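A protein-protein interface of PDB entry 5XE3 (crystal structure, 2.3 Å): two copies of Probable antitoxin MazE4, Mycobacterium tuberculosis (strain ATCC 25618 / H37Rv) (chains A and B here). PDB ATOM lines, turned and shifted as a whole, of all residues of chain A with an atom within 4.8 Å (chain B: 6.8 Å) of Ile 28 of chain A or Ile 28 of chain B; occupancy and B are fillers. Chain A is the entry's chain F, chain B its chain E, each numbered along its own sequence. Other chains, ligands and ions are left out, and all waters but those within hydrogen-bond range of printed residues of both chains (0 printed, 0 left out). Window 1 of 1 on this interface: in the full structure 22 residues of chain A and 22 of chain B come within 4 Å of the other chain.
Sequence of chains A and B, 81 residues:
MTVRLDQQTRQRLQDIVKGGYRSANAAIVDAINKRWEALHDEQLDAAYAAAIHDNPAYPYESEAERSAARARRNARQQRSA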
ATOM      1  N   VAL A   3     -25.524  12.821 -22.288  1.00  0.00           N
ATOM      2  CA  VAL A   3     -24.367  13.032 -21.383  1.00  0.00           C
ATOM      3  C   VAL A   3     -23.714  14.382 -21.649  1.00  0.00           C
ATOM      4  O   VAL A   3     -23.528  14.766 -22.809  1.00  0.00           O
ATOM      5  CB  VAL A   3     -23.286  11.900 -21.561  1.00  0.00           C
ATOM      6  CG1 VAL A   3     -21.882  12.289 -21.070  1.00  0.00           C
ATOM      7  CG2 VAL A   3     -23.752  10.617 -20.875  1.00  0.00           C
ATOM      8  N   LEU A  13     -11.803  12.365 -23.725  1.00  0.00           N
ATOM      9  CA  LEU A  13     -12.532  11.369 -24.489  1.00  0.00           C
ATOM     10  C   LEU A  13     -11.936  11.238 -25.897  1.00  0.00           C
ATOM     11  O   LEU A  13     -11.765  10.127 -26.370  1.00  0.00           O
ATOM     12  CB  LEU A  13     -14.006  11.721 -24.539  1.00  0.00           C
ATOM     13  CG  LEU A  13     -14.929  10.814 -25.327  1.00  0.00           C
ATOM     14  CD1 LEU A  13     -14.904   9.351 -24.863  1.00  0.00           C
ATOM     15  CD2 LEU A  13     -16.329  11.379 -25.174  1.00  0.00           C
ATOM     16  N   ALA A  24     -16.690   7.434 -30.032  1.00  0.00           N
ATOM     17  CA  ALA A  24     -16.926   8.024 -28.723  1.00  0.00           C
ATOM     18  C   ALA A  24     -17.761   7.086 -27.834  1.00  0.00           C
ATOM     19  O   ALA A  24     -17.437   6.829 -26.666  1.00  0.00           O
ATOM     20  CB  ALA A  24     -17.618   9.376 -28.899  1.00  0.00           C
ATOM     21  N   ASN A  25     -18.829   6.564 -28.420  1.00  0.00           N
ATOM     22  CA  ASN A  25     -19.730   5.619 -27.752  1.00  0.00           C
ATOM     23  C   ASN A  25     -19.010   4.393 -27.208  1.00  0.00           C
ATOM     24  O   ASN A  25     -19.255   3.971 -26.087  1.00  0.00           O
ATOM     25  CB  ASN A  25     -20.824   5.157 -28.723  1.00  0.00           C
ATOM     26  CG  ASN A  25     -22.004   4.519 -28.001  1.00  0.00           C
ATOM     27  OD1 ASN A  25     -22.798   5.207 -27.370  1.00  0.00           O
ATOM     28  ND2 ASN A  25     -22.129   3.199 -28.095  1.00  0.00           N
ATOM     29  N   ALA A  26     -18.127   3.833 -28.021  1.00  0.00           N
ATOM     30  CA  ALA A  26     -17.430   2.592 -27.671  1.00  0.00           C
ATOM     31  C   ALA A  26     -16.513   2.838 -26.478  1.00  0.00           C
ATOM     32  O   ALA A  26     -16.509   2.069 -25.538  1.00  0.00           O
ATOM     33  CB  ALA A  26     -16.643   2.059 -28.882  1.00  0.00           C
ATOM     34  N   ALA A  27     -15.760   3.937 -26.536  1.00  0.00           N
ATOM     35  CA  ALA A  27     -14.908   4.401 -25.436  1.00  0.00           C
ATOM     36  C   ALA A  27     -15.635   4.630 -24.104  1.00  0.00           C
ATOM     37  O   ALA A  27     -15.183   4.191 -23.066  1.00  0.00           O
ATOM     38  CB  ALA A  27     -14.161   5.638 -25.864  1.00  0.00           C
ATOM     39  N   ILE A  28     -16.787   5.255 -24.144  1.00  0.00           N
ATOM     40  CA  ILE A  28     -17.549   5.543 -22.915  1.00  0.00           C
ATOM     41  C   ILE A  28     -18.106   4.262 -22.317  1.00  0.00           C
ATOM     42  O   ILE A  28     -18.073   4.042 -21.090  1.00  0.00           O
ATOM     43  CB  ILE A  28     -18.655   6.578 -23.182  1.00  0.00           C
ATOM     44  CG1 ILE A  28     -18.016   7.933 -23.499  1.00  0.00           C
ATOM     45  CG2 ILE A  28     -19.581   6.689 -21.978  1.00  0.00           C
ATOM     46  CD1 ILE A  28     -18.972   8.965 -24.066  1.00  0.00           C
ATOM     47  N   VAL A  29     -18.574   3.390 -23.200  1.00  0.00           N
ATOM     48  CA  VAL A  29     -18.995   2.050 -22.813  1.00  0.00           C
ATOM     49  C   VAL A  29     -17.852   1.338 -22.092  1.00  0.00           C
ATOM     50  O   VAL A  29     -18.014   0.795 -20.989  1.00  0.00           O
ATOM     51  CB  VAL A  29     -19.468   1.264 -24.067  1.00  0.00           C
ATOM     52  CG1 VAL A  29     -19.535  -0.244 -23.840  1.00  0.00           C
ATOM     53  CG2 VAL A  29     -20.830   1.791 -24.514  1.00  0.00           C
ATOM     54  N   ASP A  30     -16.694   1.349 -22.711  1.00  0.00           N
ATOM     55  CA  ASP A  30     -15.555   0.713 -22.116  1.00  0.00           C
ATOM     56  C   ASP A  30     -15.081   1.367 -20.828  1.00  0.00           C
ATOM     57  O   ASP A  30     -14.727   0.663 -19.889  1.00  0.00           O
ATOM     58  CB  ASP A  30     -14.398   0.657 -23.086  1.00  0.00           C
ATOM     59  CG  ASP A  30     -13.466  -0.543 -22.796  1.00  0.00           C
ATOM     60  OD1 ASP A  30     -14.002  -1.640 -22.433  1.00  0.00           O
ATOM     61  OD2 ASP A  30     -12.228  -0.379 -22.946  1.00  0.00           O
ATOM     62  N   ALA A  31     -15.105   2.698 -20.768  1.00  0.00           N
ATOM     63  CA  ALA A  31     -14.752   3.382 -19.524  1.00  0.00           C
ATOM     64  C   ALA A  31     -15.716   3.021 -18.415  1.00  0.00           C
ATOM     65  O   ALA A  31     -15.276   2.795 -17.287  1.00  0.00           O
ATOM     66  CB  ALA A  31     -14.640   4.896 -19.728  1.00  0.00           C
ATOM     67  N   ILE A  32     -16.997   2.858 -18.733  1.00  0.00           N
ATOM     68  CA  ILE A  32     -17.987   2.525 -17.704  1.00  0.00           C
ATOM     69  C   ILE A  32     -17.692   1.130 -17.217  1.00  0.00           C
ATOM     70  O   ILE A  32     -17.670   0.858 -16.015  1.00  0.00           O
ATOM     71  CB  ILE A  32     -19.426   2.615 -18.239  1.00  0.00           C
ATOM     72  CG1 ILE A  32     -19.782   4.052 -18.591  1.00  0.00           C
ATOM     73  CG2 ILE A  32     -20.449   2.117 -17.208  1.00  0.00           C
ATOM     74  CD1 ILE A  32     -21.024   4.150 -19.465  1.00  0.00           C
ATOM     75  N   THR B   2     -25.199  12.340 -27.083  1.00  0.00           N
ATOM     76  CA  THR B   2     -26.170  11.223 -26.958  1.00  0.00           C
ATOM     77  C   THR B   2     -25.364   9.909 -26.887  1.00  0.00           C
ATOM     78  O   THR B   2     -24.568   9.645 -27.785  1.00  0.00           O
ATOM     79  CB  THR B   2     -27.155  11.175 -28.142  1.00  0.00           C
ATOM     80  N   VAL B   3     -25.560   9.121 -25.817  1.00  0.00           N
ATOM     81  CA  VAL B   3     -24.763   7.907 -25.506  1.00  0.00           C
ATOM     82  C   VAL B   3     -25.693   6.694 -25.414  1.00  0.00           C
ATOM     83  O   VAL B   3     -26.800   6.776 -24.846  1.00  0.00           O
ATOM     84  CB  VAL B   3     -23.952   8.090 -24.171  1.00  0.00           C
ATOM     85  CG1 VAL B   3     -23.664   6.786 -23.427  1.00  0.00           C
ATOM     86  CG2 VAL B   3     -22.651   8.838 -24.447  1.00  0.00           C
ATOM     87  N   LEU B   5     -26.147   2.661 -24.478  1.00  0.00           N
ATOM     88  CA  LEU B   5     -25.706   1.626 -23.582  1.00  0.00           C
ATOM     89  C   LEU B   5     -26.548   0.354 -23.726  1.00  0.00           C
ATOM     90  O   LEU B   5     -27.752   0.368 -23.493  1.00  0.00           O
ATOM     91  CB  LEU B   5     -25.795   2.102 -22.123  1.00  0.00           C
ATOM     92  CG  LEU B   5     -25.089   3.384 -21.680  1.00  0.00           C
ATOM     93  CD1 LEU B   5     -25.160   3.476 -20.171  1.00  0.00           C
ATOM     94  CD2 LEU B   5     -23.642   3.460 -22.157  1.00  0.00           C
ATOM     95  N   THR B   9     -24.189  -2.958 -19.533  1.00  0.00           N
ATOM     96  CA  THR B   9     -23.427  -1.756 -19.318  1.00  0.00           C
ATOM     97  C   THR B   9     -24.243  -0.726 -18.525  1.00  0.00           C
ATOM     98  O   THR B   9     -23.723  -0.111 -17.589  1.00  0.00           O
ATOM     99  CB  THR B   9     -22.939  -1.156 -20.649  1.00  0.00           C
ATOM    100  OG1 THR B   9     -21.857  -1.954 -21.166  1.00  0.00           O
ATOM    101  CG2 THR B   9     -22.445   0.262 -20.472  1.00  0.00           C
ATOM    102  N   LEU B  13     -23.661   0.911 -14.962  1.00  0.00           N
ATOM    103  CA  LEU B  13     -23.694   2.332 -14.643  1.00  0.00           C
ATOM    104  C   LEU B  13     -24.506   2.586 -13.372  1.00  0.00           C
ATOM    105  O   LEU B  13     -24.067   3.319 -12.490  1.00  0.00           O
ATOM    106  CB  LEU B  13     -24.263   3.105 -15.789  1.00  0.00           C
ATOM    107  CG  LEU B  13     -24.310   4.615 -15.648  1.00  0.00           C
ATOM    108  CD1 LEU B  13     -23.010   5.260 -15.193  1.00  0.00           C
ATOM    109  CD2 LEU B  13     -24.655   5.138 -17.031  1.00  0.00           C
ATOM    110  N   ILE B  16     -22.634   1.522 -10.004  1.00  0.00           N
ATOM    111  CA  ILE B  16     -21.625   2.489  -9.595  1.00  0.00           C
ATOM    112  C   ILE B  16     -22.214   3.819  -9.153  1.00  0.00           C
ATOM    113  O   ILE B  16     -21.666   4.442  -8.246  1.00  0.00           O
ATOM    114  CB  ILE B  16     -20.529   2.697 -10.659  1.00  0.00           C
ATOM    115  CG1 ILE B  16     -21.045   3.337 -11.934  1.00  0.00           C
ATOM    116  CG2 ILE B  16     -19.876   1.360 -10.972  1.00  0.00           C
ATOM    117  CD1 ILE B  16     -19.930   3.724 -12.888  1.00  0.00           C
ATOM    118  N   VAL B  17     -23.326   4.223  -9.764  1.00  0.00           N
ATOM    119  CA  VAL B  17     -24.131   5.353  -9.280  1.00  0.00           C
ATOM    120  C   VAL B  17     -24.603   5.102  -7.829  1.00  0.00           C
ATOM    121  O   VAL B  17     -24.296   5.888  -6.926  1.00  0.00           O
ATOM    122  CB  VAL B  17     -25.310   5.658 -10.245  1.00  0.00           C
ATOM    123  CG1 VAL B  17     -26.351   6.600  -9.624  1.00  0.00           C
ATOM    124  CG2 VAL B  17     -24.769   6.236 -11.545  1.00  0.00           C
ATOM    125  N   TYR B  21     -21.772   7.905  -6.411  1.00  0.00           N
ATOM    126  CA  TYR B  21     -21.853   9.012  -7.378  1.00  0.00           C
ATOM    127  C   TYR B  21     -23.191   9.751  -7.293  1.00  0.00           C
ATOM    128  O   TYR B  21     -24.210   9.217  -6.841  1.00  0.00           O
ATOM    129  CB  TYR B  21     -21.617   8.558  -8.799  1.00  0.00           C
ATOM    130  CG  TYR B  21     -20.202   8.103  -9.096  1.00  0.00           C
ATOM    131  CD1 TYR B  21     -19.823   6.783  -8.930  1.00  0.00           C
ATOM    132  CD2 TYR B  21     -19.254   8.981  -9.565  1.00  0.00           C
ATOM    133  CE1 TYR B  21     -18.539   6.350  -9.216  1.00  0.00           C
ATOM    134  CE2 TYR B  21     -17.967   8.548  -9.864  1.00  0.00           C
ATOM    135  CZ  TYR B  21     -17.620   7.235  -9.689  1.00  0.00           C
ATOM    136  OH  TYR B  21     -16.361   6.800  -9.998  1.00  0.00           O
ATOM    137  N   SER B  23     -24.889  11.381  -9.810  1.00  0.00           N
ATOM    138  CA  SER B  23     -25.783  11.108 -10.942  1.00  0.00           C
ATOM    139  C   SER B  23     -25.105  10.200 -11.968  1.00  0.00           C
ATOM    140  O   SER B  23     -23.891   9.879 -11.881  1.00  0.00           O
ATOM    141  CB  SER B  23     -26.142  12.394 -11.667  1.00  0.00           C
ATOM    142  OG  SER B  23     -25.047  12.930 -12.432  1.00  0.00           O
ATOM    143  N   ALA B  24     -25.878   9.854 -12.980  1.00  0.00           N
ATOM    144  CA  ALA B  24     -25.341   9.114 -14.118  1.00  0.00           C
ATOM    145  C   ALA B  24     -24.240   9.933 -14.818  1.00  0.00           C
ATOM    146  O   ALA B  24     -23.152   9.425 -15.160  1.00  0.00           O
ATOM    147  CB  ALA B  24     -26.465   8.756 -15.084  1.00  0.00           C
ATOM    148  N   ASN B  25     -24.518  11.213 -14.998  1.00  0.00           N
ATOM    149  CA  ASN B  25     -23.551  12.112 -15.631  1.00  0.00           C
ATOM    150  C   ASN B  25     -22.180  12.148 -14.948  1.00  0.00           C
ATOM    151  O   ASN B  25     -21.139  12.117 -15.603  1.00  0.00           O
ATOM    152  CB  ASN B  25     -24.105  13.536 -15.711  1.00  0.00           C
ATOM    153  CG  ASN B  25     -23.342  14.377 -16.713  1.00  0.00           C
ATOM    154  OD1 ASN B  25     -23.498  14.193 -17.916  1.00  0.00           O
ATOM    155  ND2 ASN B  25     -22.488  15.283 -16.228  1.00  0.00           N
ATOM    156  N   ALA B  26     -22.213  12.237 -13.628  1.00  0.00           N
ATOM    157  CA  ALA B  26     -21.001  12.385 -12.818  1.00  0.00           C
ATOM    158  C   ALA B  26     -20.158  11.087 -12.887  1.00  0.00           C
ATOM    159  O   ALA B  26     -18.949  11.141 -13.084  1.00  0.00           O
ATOM    160  CB  ALA B  26     -21.375  12.766 -11.373  1.00  0.00           C
ATOM    161  N   ALA B  27     -20.819   9.935 -12.753  1.00  0.00           N
ATOM    162  CA  ALA B  27     -20.178   8.620 -12.958  1.00  0.00           C
ATOM    163  C   ALA B  27     -19.484   8.442 -14.310  1.00  0.00           C
ATOM    164  O   ALA B  27     -18.336   8.068 -14.351  1.00  0.00           O
ATOM    165  CB  ALA B  27     -21.174   7.523 -12.726  1.00  0.00           C
ATOM    166  N   ILE B  28     -20.139   8.797 -15.400  1.00  0.00           N
ATOM    167  CA  ILE B  28     -19.554   8.636 -16.753  1.00  0.00           C
ATOM    168  C   ILE B  28     -18.375   9.544 -16.951  1.00  0.00           C
ATOM    169  O   ILE B  28     -17.350   9.144 -17.505  1.00  0.00           O
ATOM    170  CB  ILE B  28     -20.612   8.878 -17.835  1.00  0.00           C
ATOM    171  CG1 ILE B  28     -21.579   7.681 -17.865  1.00  0.00           C
ATOM    172  CG2 ILE B  28     -19.967   9.091 -19.190  1.00  0.00           C
ATOM    173  CD1 ILE B  28     -22.954   7.971 -18.450  1.00  0.00           C
ATOM    174  N   VAL B  29     -18.535  10.774 -16.482  1.00  0.00           N
ATOM    175  CA  VAL B  29     -17.436  11.732 -16.380  1.00  0.00           C
ATOM    176  C   VAL B  29     -16.230  11.151 -15.605  1.00  0.00           C
ATOM    177  O   VAL B  29     -15.072  11.257 -16.035  1.00  0.00           O
ATOM    178  CB  VAL B  29     -17.969  13.042 -15.720  1.00  0.00           C
ATOM    179  CG1 VAL B  29     -16.858  13.913 -15.126  1.00  0.00           C
ATOM    180  CG2 VAL B  29     -18.774  13.827 -16.758  1.00  0.00           C
ATOM    181  N   ASP B  30     -16.499  10.534 -14.469  1.00  0.00           N
ATOM    182  CA  ASP B  30     -15.434   9.936 -13.720  1.00  0.00           C
ATOM    183  C   ASP B  30     -14.828   8.686 -14.377  1.00  0.00           C
ATOM    184  O   ASP B  30     -13.612   8.514 -14.366  1.00  0.00           O
ATOM    185  CB  ASP B  30     -15.899   9.578 -12.332  1.00  0.00           C
ATOM    186  CG  ASP B  30     -14.742   9.551 -11.330  1.00  0.00           C
ATOM    187  OD1 ASP B  30     -13.805  10.419 -11.476  1.00  0.00           O
ATOM    188  OD2 ASP B  30     -14.797   8.690 -10.400  1.00  0.00           O
ATOM    189  N   ALA B  31     -15.662   7.833 -14.952  1.00  0.00           N
ATOM    190  CA  ALA B  31     -15.145   6.692 -15.697  1.00  0.00           C
ATOM    191  C   ALA B  31     -14.296   7.166 -16.883  1.00  0.00           C
ATOM    192  O   ALA B  31     -13.239   6.579 -17.129  1.00  0.00           O
ATOM    193  CB  ALA B  31     -16.269   5.751 -16.142  1.00  0.00           C
ATOM    194  N   ILE B  32     -14.670   8.268 -17.544  1.00  0.00           N
ATOM    195  CA  ILE B  32     -13.855   8.716 -18.679  1.00  0.00           C
ATOM    196  C   ILE B  32     -12.517   9.205 -18.151  1.00  0.00           C
ATOM    197  O   ILE B  32     -11.466   8.817 -18.640  1.00  0.00           O
ATOM    198  CB  ILE B  32     -14.521   9.819 -19.531  1.00  0.00           C
ATOM    199  CG1 ILE B  32     -15.812   9.318 -20.172  1.00  0.00           C
ATOM    200  CG2 ILE B  32     -13.560  10.292 -20.622  1.00  0.00           C
ATOM    201  CD1 ILE B  32     -16.765  10.431 -20.526  1.00  0.00           C
ATOM    202  N   ASN B  33     -12.562  10.052 -17.129  1.00  0.00           N
ATOM    203  CA  ASN B  33     -11.318  10.554 -16.534  1.00  0.00           C
ATOM    204  C   ASN B  33     -10.421   9.479 -15.959  1.00  0.00           C
ATOM    205  O   ASN B  33      -9.226   9.531 -16.152  1.00  0.00           O
ATOM    206  CB  ASN B  33     -11.618  11.601 -15.471  1.00  0.00           C
ATOM    207  CG  ASN B  33     -11.916  12.943 -16.093  1.00  0.00           C
ATOM    208  OD1 ASN B  33     -11.084  13.491 -16.809  1.00  0.00           O
ATOM    209  ND2 ASN B  33     -13.097  13.433 -15.896  1.00  0.00           N
ATOM    210  N   LYS B  34     -11.002   8.491 -15.297  1.00  0.00           N
ATOM    211  CA  LYS B  34     -10.220   7.388 -14.783  1.00  0.00           C
ATOM    212  C   LYS B  34      -9.632   6.499 -15.879  1.00  0.00           C
ATOM    213  O   LYS B  34      -8.504   6.055 -15.760  1.00  0.00           O
ATOM    214  CB  LYS B  34     -11.031   6.572 -13.763  1.00  0.00           C
ATOM    215  CG  LYS B  34     -10.832   7.176 -12.374  1.00  0.00           C
ATOM    216  CD  LYS B  34     -11.791   6.636 -11.348  1.00  0.00           C
ATOM    217  CE  LYS B  34     -11.306   6.878  -9.920  1.00  0.00           C
ATOM    218  NZ  LYS B  34     -10.892   8.276  -9.771  1.00  0.00           N
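The side-chain hydroxyl (OG) of Ser 23 of chain B is in hydrogen-bond range of the backbone NH (N) of Asn 25 of chain B, at 3.1 Å.
Among the printed residues, merely in contact across the chains: Val 3 of chain A with Asn 25 of chain B, Val 3 of chain A with Ile 28 of chain B, Asn 25 of chain A with Val 3 of chain B, Ile 28 of chain A with Val 3 of chain B, Ile 28 of chain A with Ile 28 of chain B, Val 29 of chain A with Thr 9 of chain B, Ala 31 of chain A with Ala 31 of chain B, Ile 32 of chain A with Leu 5 of chain B, Ile 32 of chain A with Thr 9 of chain B, Ile 32 of chain A with Ile 28 of chain B and Ile 32 of chain A with Ala 31 of chain B.
Ile 28 of chain A touches just these residues of chain B: Val 3 (3.7 Å) and Ile 28 (3.7 Å). Printed residues of chain B within 4 Å of Ala 31 of chain A: Ala 31. Of the printed residues of chain B, Ile 32 of chain A touches Leu 5, Thr 9, Ile 28 and Ala 31. Of the printed residues of chain A, Leu 5 of chain B touches Ile 32. Ile 16 of chain B touches none of the printed residues of chain A. Tyr 21 of chain B touches none of the printed residues of chain A. Of chain A, only Val 3, Ile 28 and Ile 32 come within 4 Å of Ile 28 of chain B. The nearest printed residue of chain A that does not touch Ile 28 of chain B is Ala 31 of chain A (5.5 Å). The nearest printed residue of chain A that does not touch Thr 9 of chain B is Ile 28 of chain A (5.8 Å).
Hydrophobic or aromatic side chains of chain B within 4 Å of the printed part of chain A: Val 3, Leu 5, Ile 28 and Ala 31. Of the 11 printed residues of chain A, 6 touch a printed residue of chain B. Hydrophobic or aromatic side chains of chain A within 4 Å of the printed part of chain B: Val 3, Ile 28, Val 29, Ala 31 and Ile 32. Among the printed residues, 11 pairs touch across the chains. Among the printed residues, no Asp or Glu carboxylate lies within 4 Å of a Lys or Arg side-chain nitrogen of the other chain.
Val 3 of chain A touches Asn 25 of chain B, and with the chains exchanged Asn 25 of chain A touches Val 3 of chain B. Ile 28 of chain A touches its own counterpart, Ile 28 of chain B. Ala 31 of chain B touches its own counterpart, Ala 31 of chain A. Ile 32 of chain A touches Ile 28 of chain B, but with the chains exchanged Ile 28 of chain A does not touch Ile 32 of chain B (4.1 Å). Positions printed for both chains: 3, 13, 24, 25, 26, 27, 28, 29, 30, 31 and 32.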
